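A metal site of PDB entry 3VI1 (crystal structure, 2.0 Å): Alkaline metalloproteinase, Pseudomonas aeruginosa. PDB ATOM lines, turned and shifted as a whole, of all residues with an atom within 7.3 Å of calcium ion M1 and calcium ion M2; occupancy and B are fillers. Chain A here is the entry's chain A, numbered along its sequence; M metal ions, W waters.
Seven residues have an atom within 4 Å of calcium ion M1: Asn 343, Val 345, Asn 347, Gly 360, Gly 361, Leu 362 and Asp 365. The nearest printed residue that does not touch calcium ion M1 is Asp 344 (4.1 Å).
Water W1 lies within hydrogen-bond range of OD2 of Asp 390 (2.6 Å) and N of Gly 361 (3.3 Å).
O of Asn 343 is bound to calcium ion M1 (2.3 Å). O of Leu 362 binds calcium ion M1, at 2.4 Å. The side-chain amide oxygen (OD1) of Asn 347 is bound to calcium ion M1 (2.4 Å). Calcium ion M1 is bound by O of Val 345, 2.4 Å away. The backbone carbonyl oxygen (O) of Gly 360 binds calcium ion M1, at 2.4 Å. OD1 of Asp 365 is bound to calcium ion M1.
The side-chain carboxylate (OE2) of Glu 383 is in hydrogen-bond range of the backbone NH (N) of Asp 380, 3.3 Å away. OH of Tyr 378 is in hydrogen-bond range of OD2 of Asp 390 (3.2 Å). The side-chain carboxylate of Glu 383 is in hydrogen-bond range of the side-chain hydroxyl of Tyr 359. The backbone carbonyl oxygen (O) of Asn 347 is in hydrogen-bond range of the backbone NH (N) of Gln 366 (2.8 Å). ND2 of Asn 347 sits at hydrogen-bond distance from O of Glu 329. O of Leu 305 sits at hydrogen-bond distance from ND2 of Asn 343, at 2.8 Å. OG of Ser 384 is in hydrogen-bond range of N of Asp 390 (2.8 Å). The side-chain amide oxygen of Asn 343 lies close to the backbone NH of Val 345.
Calcium ion M2 is bound by the side-chain carboxylate (OD2) of Asp 365 (2.3 Å), the backbone carbonyl oxygen (O) of Glu 383 (2.3 Å), water W1 (2.3 Å), the backbone carbonyl oxygen (O) of Gly 361 (2.4 Å), the backbone carbonyl oxygen (O) of Gly 363 (2.4 Å) and the side-chain carboxylate (OD1) of Asp 390 (2.6 Å). Calcium ion M2 has six donor atoms within binding distance.
Of the 30 residues printed, 6 come within 4 Å of calcium ion M2.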
ATOM      1  N   LEU A 305      11.527 -21.401  26.384  1.00  0.00           N
ATOM      2  CA  LEU A 305      12.590 -22.416  26.367  1.00  0.00           C
ATOM      3  C   LEU A 305      13.865 -22.011  25.624  1.00  0.00           C
ATOM      4  O   LEU A 305      14.850 -22.758  25.630  1.00  0.00           O
ATOM      5  CB  LEU A 305      12.058 -23.759  25.841  1.00  0.00           C
ATOM      6  CG  LEU A 305      11.152 -24.594  26.757  1.00  0.00           C
ATOM      7  CD1 LEU A 305      10.831 -25.929  26.111  1.00  0.00           C
ATOM      8  CD2 LEU A 305      11.766 -24.823  28.140  1.00  0.00           C
ATOM      9  N   GLU A 329      14.903 -28.793  26.801  1.00  0.00           N
ATOM     10  CA  GLU A 329      14.044 -29.425  25.806  1.00  0.00           C
ATOM     11  C   GLU A 329      12.548 -29.299  26.080  1.00  0.00           C
ATOM     12  O   GLU A 329      11.773 -29.020  25.166  1.00  0.00           O
ATOM     13  CB  GLU A 329      14.404 -30.912  25.654  1.00  0.00           C
ATOM     14  CG  GLU A 329      15.708 -31.172  24.895  1.00  0.00           C
ATOM     15  CD  GLU A 329      16.950 -30.762  25.666  1.00  0.00           C
ATOM     16  OE1 GLU A 329      16.934 -30.764  26.917  1.00  0.00           O
ATOM     17  OE2 GLU A 329      17.982 -30.445  25.024  1.00  0.00           O
ATOM     18  N   ILE A 341       6.462 -21.379  24.999  1.00  0.00           N
ATOM     19  CA  ILE A 341       7.258 -21.155  23.796  1.00  0.00           C
ATOM     20  C   ILE A 341       8.482 -22.080  23.786  1.00  0.00           C
ATOM     21  O   ILE A 341       9.293 -22.066  24.714  1.00  0.00           O
ATOM     22  CB  ILE A 341       7.693 -19.668  23.647  1.00  0.00           C
ATOM     23  CG1 ILE A 341       6.454 -18.757  23.599  1.00  0.00           C
ATOM     24  CG2 ILE A 341       8.551 -19.485  22.392  1.00  0.00           C
ATOM     25  CD1 ILE A 341       6.759 -17.268  23.536  1.00  0.00           C
ATOM     26  N   GLY A 342       8.579 -22.886  22.730  1.00  0.00           N
ATOM     27  CA  GLY A 342       9.717 -23.790  22.543  1.00  0.00           C
ATOM     28  C   GLY A 342      10.896 -23.101  21.872  1.00  0.00           C
ATOM     29  O   GLY A 342      10.841 -21.909  21.575  1.00  0.00           O
ATOM     30  N   ASN A 343      11.951 -23.868  21.648  1.00  0.00           N
ATOM     31  CA  ASN A 343      13.164 -23.358  20.999  1.00  0.00           C
ATOM     32  C   ASN A 343      13.434 -24.056  19.660  1.00  0.00           C
ATOM     33  O   ASN A 343      12.513 -24.627  19.067  1.00  0.00           O
ATOM     34  CB  ASN A 343      14.373 -23.448  21.949  1.00  0.00           C
ATOM     35  CG  ASN A 343      14.549 -24.831  22.549  1.00  0.00           C
ATOM     36  OD1 ASN A 343      14.266 -25.844  21.912  1.00  0.00           O
ATOM     37  ND2 ASN A 343      15.030 -24.880  23.783  1.00  0.00           N
ATOM     38  N   ASP A 344      14.682 -24.025  19.218  1.00  0.00           N
ATOM     39  CA  ASP A 344      15.036 -24.527  17.890  1.00  0.00           C
ATOM     40  C   ASP A 344      15.038 -26.056  17.756  1.00  0.00           C
ATOM     41  O   ASP A 344      14.868 -26.578  16.649  1.00  0.00           O
ATOM     42  CB  ASP A 344      16.357 -23.926  17.414  1.00  0.00           C
ATOM     43  CG  ASP A 344      16.213 -22.485  16.972  1.00  0.00           C
ATOM     44  OD1 ASP A 344      15.100 -21.916  17.094  1.00  0.00           O
ATOM     45  OD2 ASP A 344      17.210 -21.896  16.488  1.00  0.00           O
ATOM     46  N   VAL A 345      15.232 -26.764  18.863  1.00  0.00           N
ATOM     47  CA  VAL A 345      15.259 -28.235  18.834  1.00  0.00           C
ATOM     48  C   VAL A 345      13.873 -28.842  19.110  1.00  0.00           C
ATOM     49  O   VAL A 345      12.900 -28.112  19.319  1.00  0.00           O
ATOM     50  CB  VAL A 345      16.321 -28.826  19.822  1.00  0.00           C
ATOM     51  CG1 VAL A 345      17.720 -28.338  19.478  1.00  0.00           C
ATOM     52  CG2 VAL A 345      15.974 -28.519  21.277  1.00  0.00           C
ATOM     53  N   ALA A 346      13.797 -30.169  19.081  1.00  0.00           N
ATOM     54  CA  ALA A 346      12.564 -30.895  19.358  1.00  0.00           C
ATOM     55  C   ALA A 346      12.135 -30.677  20.808  1.00  0.00           C
ATOM     56  O   ALA A 346      12.897 -30.945  21.736  1.00  0.00           O
ATOM     57  CB  ALA A 346      12.731 -32.382  19.063  1.00  0.00           C
ATOM     58  N   ASN A 347      10.909 -30.183  20.989  1.00  0.00           N
ATOM     59  CA  ASN A 347      10.385 -29.896  22.329  1.00  0.00           C
ATOM     60  C   ASN A 347       9.130 -30.690  22.668  1.00  0.00           C
ATOM     61  O   ASN A 347       8.258 -30.888  21.823  1.00  0.00           O
ATOM     62  CB  ASN A 347      10.065 -28.394  22.465  1.00  0.00           C
ATOM     63  CG  ASN A 347      11.271 -27.505  22.205  1.00  0.00           C
ATOM     64  OD1 ASN A 347      11.215 -26.624  21.354  1.00  0.00           O
ATOM     65  ND2 ASN A 347      12.350 -27.722  22.934  1.00  0.00           N
ATOM     66  N   VAL A 348       9.051 -31.140  23.917  1.00  0.00           N
ATOM     67  CA  VAL A 348       7.808 -31.664  24.465  1.00  0.00           C
ATOM     68  C   VAL A 348       7.176 -30.565  25.306  1.00  0.00           C
ATOM     69  O   VAL A 348       7.709 -30.168  26.342  1.00  0.00           O
ATOM     70  CB  VAL A 348       8.023 -32.945  25.317  1.00  0.00           C
ATOM     71  CG1 VAL A 348       6.687 -33.455  25.865  1.00  0.00           C
ATOM     72  CG2 VAL A 348       8.702 -34.044  24.498  1.00  0.00           C
ATOM     73  N   LEU A 349       6.045 -30.046  24.829  1.00  0.00           N
ATOM     74  CA  LEU A 349       5.321 -28.995  25.551  1.00  0.00           C
ATOM     75  C   LEU A 349       3.992 -29.519  26.061  1.00  0.00           C
ATOM     76  O   LEU A 349       3.169 -30.025  25.290  1.00  0.00           O
ATOM     77  CB  LEU A 349       5.108 -27.765  24.655  1.00  0.00           C
ATOM     78  CG  LEU A 349       6.333 -27.011  24.096  1.00  0.00           C
ATOM     79  CD1 LEU A 349       5.873 -25.886  23.186  1.00  0.00           C
ATOM     80  CD2 LEU A 349       7.231 -26.479  25.205  1.00  0.00           C
ATOM     81  N   TYR A 359       3.617 -22.914  21.352  1.00  0.00           N
ATOM     82  CA  TYR A 359       4.403 -22.526  20.180  1.00  0.00           C
ATOM     83  C   TYR A 359       5.681 -23.352  20.147  1.00  0.00           C
ATOM     84  O   TYR A 359       6.655 -23.036  20.835  1.00  0.00           O
ATOM     85  CB  TYR A 359       4.717 -21.028  20.228  1.00  0.00           C
ATOM     86  CG  TYR A 359       5.349 -20.469  18.976  1.00  0.00           C
ATOM     87  CD1 TYR A 359       6.735 -20.330  18.871  1.00  0.00           C
ATOM     88  CD2 TYR A 359       4.554 -20.047  17.908  1.00  0.00           C
ATOM     89  CE1 TYR A 359       7.313 -19.809  17.715  1.00  0.00           C
ATOM     90  CE2 TYR A 359       5.128 -19.519  16.755  1.00  0.00           C
ATOM     91  CZ  TYR A 359       6.503 -19.405  16.665  1.00  0.00           C
ATOM     92  OH  TYR A 359       7.067 -18.874  15.523  1.00  0.00           O
ATOM     93  N   GLY A 360       5.665 -24.404  19.343  1.00  0.00           N
ATOM     94  CA  GLY A 360       6.782 -25.333  19.258  1.00  0.00           C
ATOM     95  C   GLY A 360       8.066 -24.718  18.717  1.00  0.00           C
ATOM     96  O   GLY A 360       9.162 -25.083  19.148  1.00  0.00           O
ATOM     97  N   GLY A 361       7.927 -23.777  17.788  1.00  0.00           N
ATOM     98  CA  GLY A 361       9.065 -23.180  17.111  1.00  0.00           C
ATOM     99  C   GLY A 361       9.649 -24.144  16.101  1.00  0.00           C
ATOM    100  O   GLY A 361       8.948 -25.018  15.598  1.00  0.00           O
ATOM    101  N   LEU A 362      10.945 -23.992  15.808  1.00  0.00           N
ATOM    102  CA  LEU A 362      11.626 -24.867  14.864  1.00  0.00           C
ATOM    103  C   LEU A 362      11.775 -26.290  15.421  1.00  0.00           C
ATOM    104  O   LEU A 362      11.764 -26.492  16.635  1.00  0.00           O
ATOM    105  CB  LEU A 362      12.995 -24.284  14.472  1.00  0.00           C
ATOM    106  CG  LEU A 362      12.993 -22.974  13.678  1.00  0.00           C
ATOM    107  CD1 LEU A 362      14.336 -22.264  13.809  1.00  0.00           C
ATOM    108  CD2 LEU A 362      12.634 -23.179  12.216  1.00  0.00           C
ATOM    109  N   GLY A 363      11.903 -27.260  14.524  1.00  0.00           N
ATOM    110  CA  GLY A 363      12.011 -28.673  14.899  1.00  0.00           C
ATOM    111  C   GLY A 363      10.668 -29.388  14.921  1.00  0.00           C
ATOM    112  O   GLY A 363       9.621 -28.751  14.780  1.00  0.00           O
ATOM    113  N   ALA A 364      10.715 -30.701  15.085  1.00  0.00           N
ATOM    114  CA  ALA A 364       9.498 -31.516  15.213  1.00  0.00           C
ATOM    115  C   ALA A 364       9.137 -31.644  16.686  1.00  0.00           C
ATOM    116  O   ALA A 364       9.807 -32.341  17.446  1.00  0.00           O
ATOM    117  CB  ALA A 364       9.701 -32.873  14.577  1.00  0.00           C
ATOM    118  N   ASP A 365       8.053 -30.968  17.087  1.00  0.00           N
ATOM    119  CA  ASP A 365       7.679 -30.875  18.498  1.00  0.00           C
ATOM    120  C   ASP A 365       6.493 -31.761  18.871  1.00  0.00           C
ATOM    121  O   ASP A 365       5.595 -31.988  18.058  1.00  0.00           O
ATOM    122  CB  ASP A 365       7.378 -29.422  18.873  1.00  0.00           C
ATOM    123  CG  ASP A 365       8.498 -28.481  18.496  1.00  0.00           C
ATOM    124  OD1 ASP A 365       9.564 -28.494  19.148  1.00  0.00           O
ATOM    125  OD2 ASP A 365       8.304 -27.700  17.535  1.00  0.00           O
ATOM    126  N   GLN A 366       6.513 -32.250  20.101  1.00  0.00           N
ATOM    127  CA  GLN A 366       5.411 -33.028  20.658  1.00  0.00           C
ATOM    128  C   GLN A 366       4.578 -32.115  21.546  1.00  0.00           C
ATOM    129  O   GLN A 366       5.026 -31.692  22.615  1.00  0.00           O
ATOM    130  CB  GLN A 366       5.938 -34.236  21.436  1.00  0.00           C
ATOM    131  CG  GLN A 366       7.025 -35.047  20.723  1.00  0.00           C
ATOM    132  CD  GLN A 366       6.606 -35.515  19.334  1.00  0.00           C
ATOM    133  OE1 GLN A 366       7.320 -35.308  18.349  1.00  0.00           O
ATOM    134  NE2 GLN A 366       5.442 -36.140  19.237  1.00  0.00           N
ATOM    135  N   LEU A 367       3.366 -31.801  21.099  1.00  0.00           N
ATOM    136  CA  LEU A 367       2.544 -30.789  21.754  1.00  0.00           C
ATOM    137  C   LEU A 367       1.302 -31.351  22.426  1.00  0.00           C
ATOM    138  O   LEU A 367       0.388 -31.869  21.760  1.00  0.00           O
ATOM    139  CB  LEU A 367       2.190 -29.653  20.782  1.00  0.00           C
ATOM    140  CG  LEU A 367       3.338 -28.991  20.013  1.00  0.00           C
ATOM    141  CD1 LEU A 367       2.813 -27.864  19.132  1.00  0.00           C
ATOM    142  CD2 LEU A 367       4.433 -28.466  20.944  1.00  0.00           C
ATOM    143  N   VAL A 377       0.151 -22.724  17.879  1.00  0.00           N
ATOM    144  CA  VAL A 377       0.452 -21.575  17.025  1.00  0.00           C
ATOM    145  C   VAL A 377       1.672 -21.805  16.146  1.00  0.00           C
ATOM    146  O   VAL A 377       2.664 -22.407  16.577  1.00  0.00           O
ATOM    147  CB  VAL A 377       0.629 -20.278  17.869  1.00  0.00           C
ATOM    148  CG1 VAL A 377       1.071 -19.096  17.018  1.00  0.00           C
ATOM    149  CG2 VAL A 377      -0.660 -19.936  18.604  1.00  0.00           C
ATOM    150  N   TYR A 378       1.595 -21.328  14.907  1.00  0.00           N
ATOM    151  CA  TYR A 378       2.684 -21.433  13.941  1.00  0.00           C
ATOM    152  C   TYR A 378       2.954 -20.087  13.275  1.00  0.00           C
ATOM    153  O   TYR A 378       2.052 -19.470  12.710  1.00  0.00           O
ATOM    154  CB  TYR A 378       2.373 -22.534  12.916  1.00  0.00           C
ATOM    155  CG  TYR A 378       2.189 -23.892  13.545  1.00  0.00           C
ATOM    156  CD1 TYR A 378       0.931 -24.318  13.982  1.00  0.00           C
ATOM    157  CD2 TYR A 378       3.267 -24.754  13.728  1.00  0.00           C
ATOM    158  CE1 TYR A 378       0.757 -25.567  14.577  1.00  0.00           C
ATOM    159  CE2 TYR A 378       3.110 -26.006  14.319  1.00  0.00           C
ATOM    160  CZ  TYR A 378       1.852 -26.399  14.738  1.00  0.00           C
ATOM    161  OH  TYR A 378       1.688 -27.637  15.321  1.00  0.00           O
ATOM    162  N   ASP A 380       5.892 -19.692  11.251  1.00  0.00           N
ATOM    163  CA  ASP A 380       6.696 -19.976  10.062  1.00  0.00           C
ATOM    164  C   ASP A 380       6.453 -21.394   9.561  1.00  0.00           C
ATOM    165  O   ASP A 380       6.194 -22.305  10.350  1.00  0.00           O
ATOM    166  CB  ASP A 380       8.188 -19.767  10.362  1.00  0.00           C
ATOM    167  CG  ASP A 380       9.015 -19.553   9.111  1.00  0.00           C
ATOM    168  OD1 ASP A 380       9.089 -20.466   8.270  1.00  0.00           O
ATOM    169  OD2 ASP A 380       9.594 -18.454   8.976  1.00  0.00           O
ATOM    170  N   ALA A 382       8.634 -23.416   8.154  1.00  0.00           N
ATOM    171  CA  ALA A 382       9.777 -24.256   8.551  1.00  0.00           C
ATOM    172  C   ALA A 382       9.632 -24.864   9.948  1.00  0.00           C
ATOM    173  O   ALA A 382      10.357 -25.787  10.311  1.00  0.00           O
ATOM    174  CB  ALA A 382      11.069 -23.451   8.443  1.00  0.00           C
ATOM    175  N   GLU A 383       8.690 -24.333  10.729  1.00  0.00           N
ATOM    176  CA  GLU A 383       8.438 -24.803  12.087  1.00  0.00           C
ATOM    177  C   GLU A 383       7.792 -26.192  12.122  1.00  0.00           C
ATOM    178  O   GLU A 383       7.907 -26.911  13.123  1.00  0.00           O
ATOM    179  CB  GLU A 383       7.598 -23.791  12.869  1.00  0.00           C
ATOM    180  CG  GLU A 383       8.370 -22.528  13.232  1.00  0.00           C
ATOM    181  CD  GLU A 383       7.482 -21.375  13.662  1.00  0.00           C
ATOM    182  OE1 GLU A 383       6.278 -21.599  13.947  1.00  0.00           O
ATOM    183  OE2 GLU A 383       7.989 -20.248  13.715  1.00  0.00           O
ATOM    184  N   SER A 384       7.108 -26.570  11.044  1.00  0.00           N
ATOM    185  CA  SER A 384       6.549 -27.906  10.915  1.00  0.00           C
ATOM    186  C   SER A 384       6.616 -28.364   9.456  1.00  0.00           C
ATOM    187  O   SER A 384       5.659 -28.219   8.699  1.00  0.00           O
ATOM    188  CB  SER A 384       5.113 -27.944  11.451  1.00  0.00           C
ATOM    189  OG  SER A 384       4.751 -29.253  11.854  1.00  0.00           O
ATOM    190  N   SER A 385       7.775 -28.904   9.082  1.00  0.00           N
ATOM    191  CA  SER A 385       8.029 -29.362   7.713  1.00  0.00           C
ATOM    192  C   SER A 385       7.208 -30.592   7.357  1.00  0.00           C
ATOM    193  O   SER A 385       6.771 -31.338   8.248  1.00  0.00           O
ATOM    194  CB  SER A 385       9.521 -29.660   7.532  1.00  0.00           C
ATOM    195  OG  SER A 385       9.949 -30.687   8.411  1.00  0.00           O
ATOM    196  N   ALA A 388       9.292 -33.668   8.544  1.00  0.00           N
ATOM    197  CA  ALA A 388       9.448 -33.803   9.988  1.00  0.00           C
ATOM    198  C   ALA A 388       8.473 -32.885  10.748  1.00  0.00           C
ATOM    199  O   ALA A 388       8.883 -31.887  11.348  1.00  0.00           O
ATOM    200  CB  ALA A 388      10.891 -33.529  10.402  1.00  0.00           C
ATOM    201  N   PRO A 389       7.168 -33.228  10.731  1.00  0.00           N
ATOM    202  CA  PRO A 389       6.146 -32.351  11.304  1.00  0.00           C
ATOM    203  C   PRO A 389       5.979 -32.473  12.813  1.00  0.00           C
ATOM    204  O   PRO A 389       6.431 -33.443  13.432  1.00  0.00           O
ATOM    205  CB  PRO A 389       4.877 -32.820  10.600  1.00  0.00           C
ATOM    206  CG  PRO A 389       5.099 -34.260  10.314  1.00  0.00           C
ATOM    207  CD  PRO A 389       6.586 -34.452  10.162  1.00  0.00           C
ATOM    208  N   ASP A 390       5.326 -31.464  13.397  1.00  0.00           N
ATOM    209  CA  ASP A 390       4.853 -31.504  14.779  1.00  0.00           C
ATOM    210  C   ASP A 390       3.817 -32.592  14.948  1.00  0.00           C
ATOM    211  O   ASP A 390       3.162 -32.998  13.978  1.00  0.00           O
ATOM    212  CB  ASP A 390       4.184 -30.169  15.142  1.00  0.00           C
ATOM    213  CG  ASP A 390       5.174 -29.110  15.591  1.00  0.00           C
ATOM    214  OD1 ASP A 390       6.397 -29.259  15.358  1.00  0.00           O
ATOM    215  OD2 ASP A 390       4.717 -28.100  16.177  1.00  0.00           O
HETATM  216 CA    CA M   1      11.128 -26.495  18.947  1.00  0.00          CA
HETATM  217 CA    CA M   2       7.992 -27.157  15.373  1.00  0.00          CA
HETATM  218  O   HOH W   1       6.159 -25.936  16.013  1.00  0.00           O
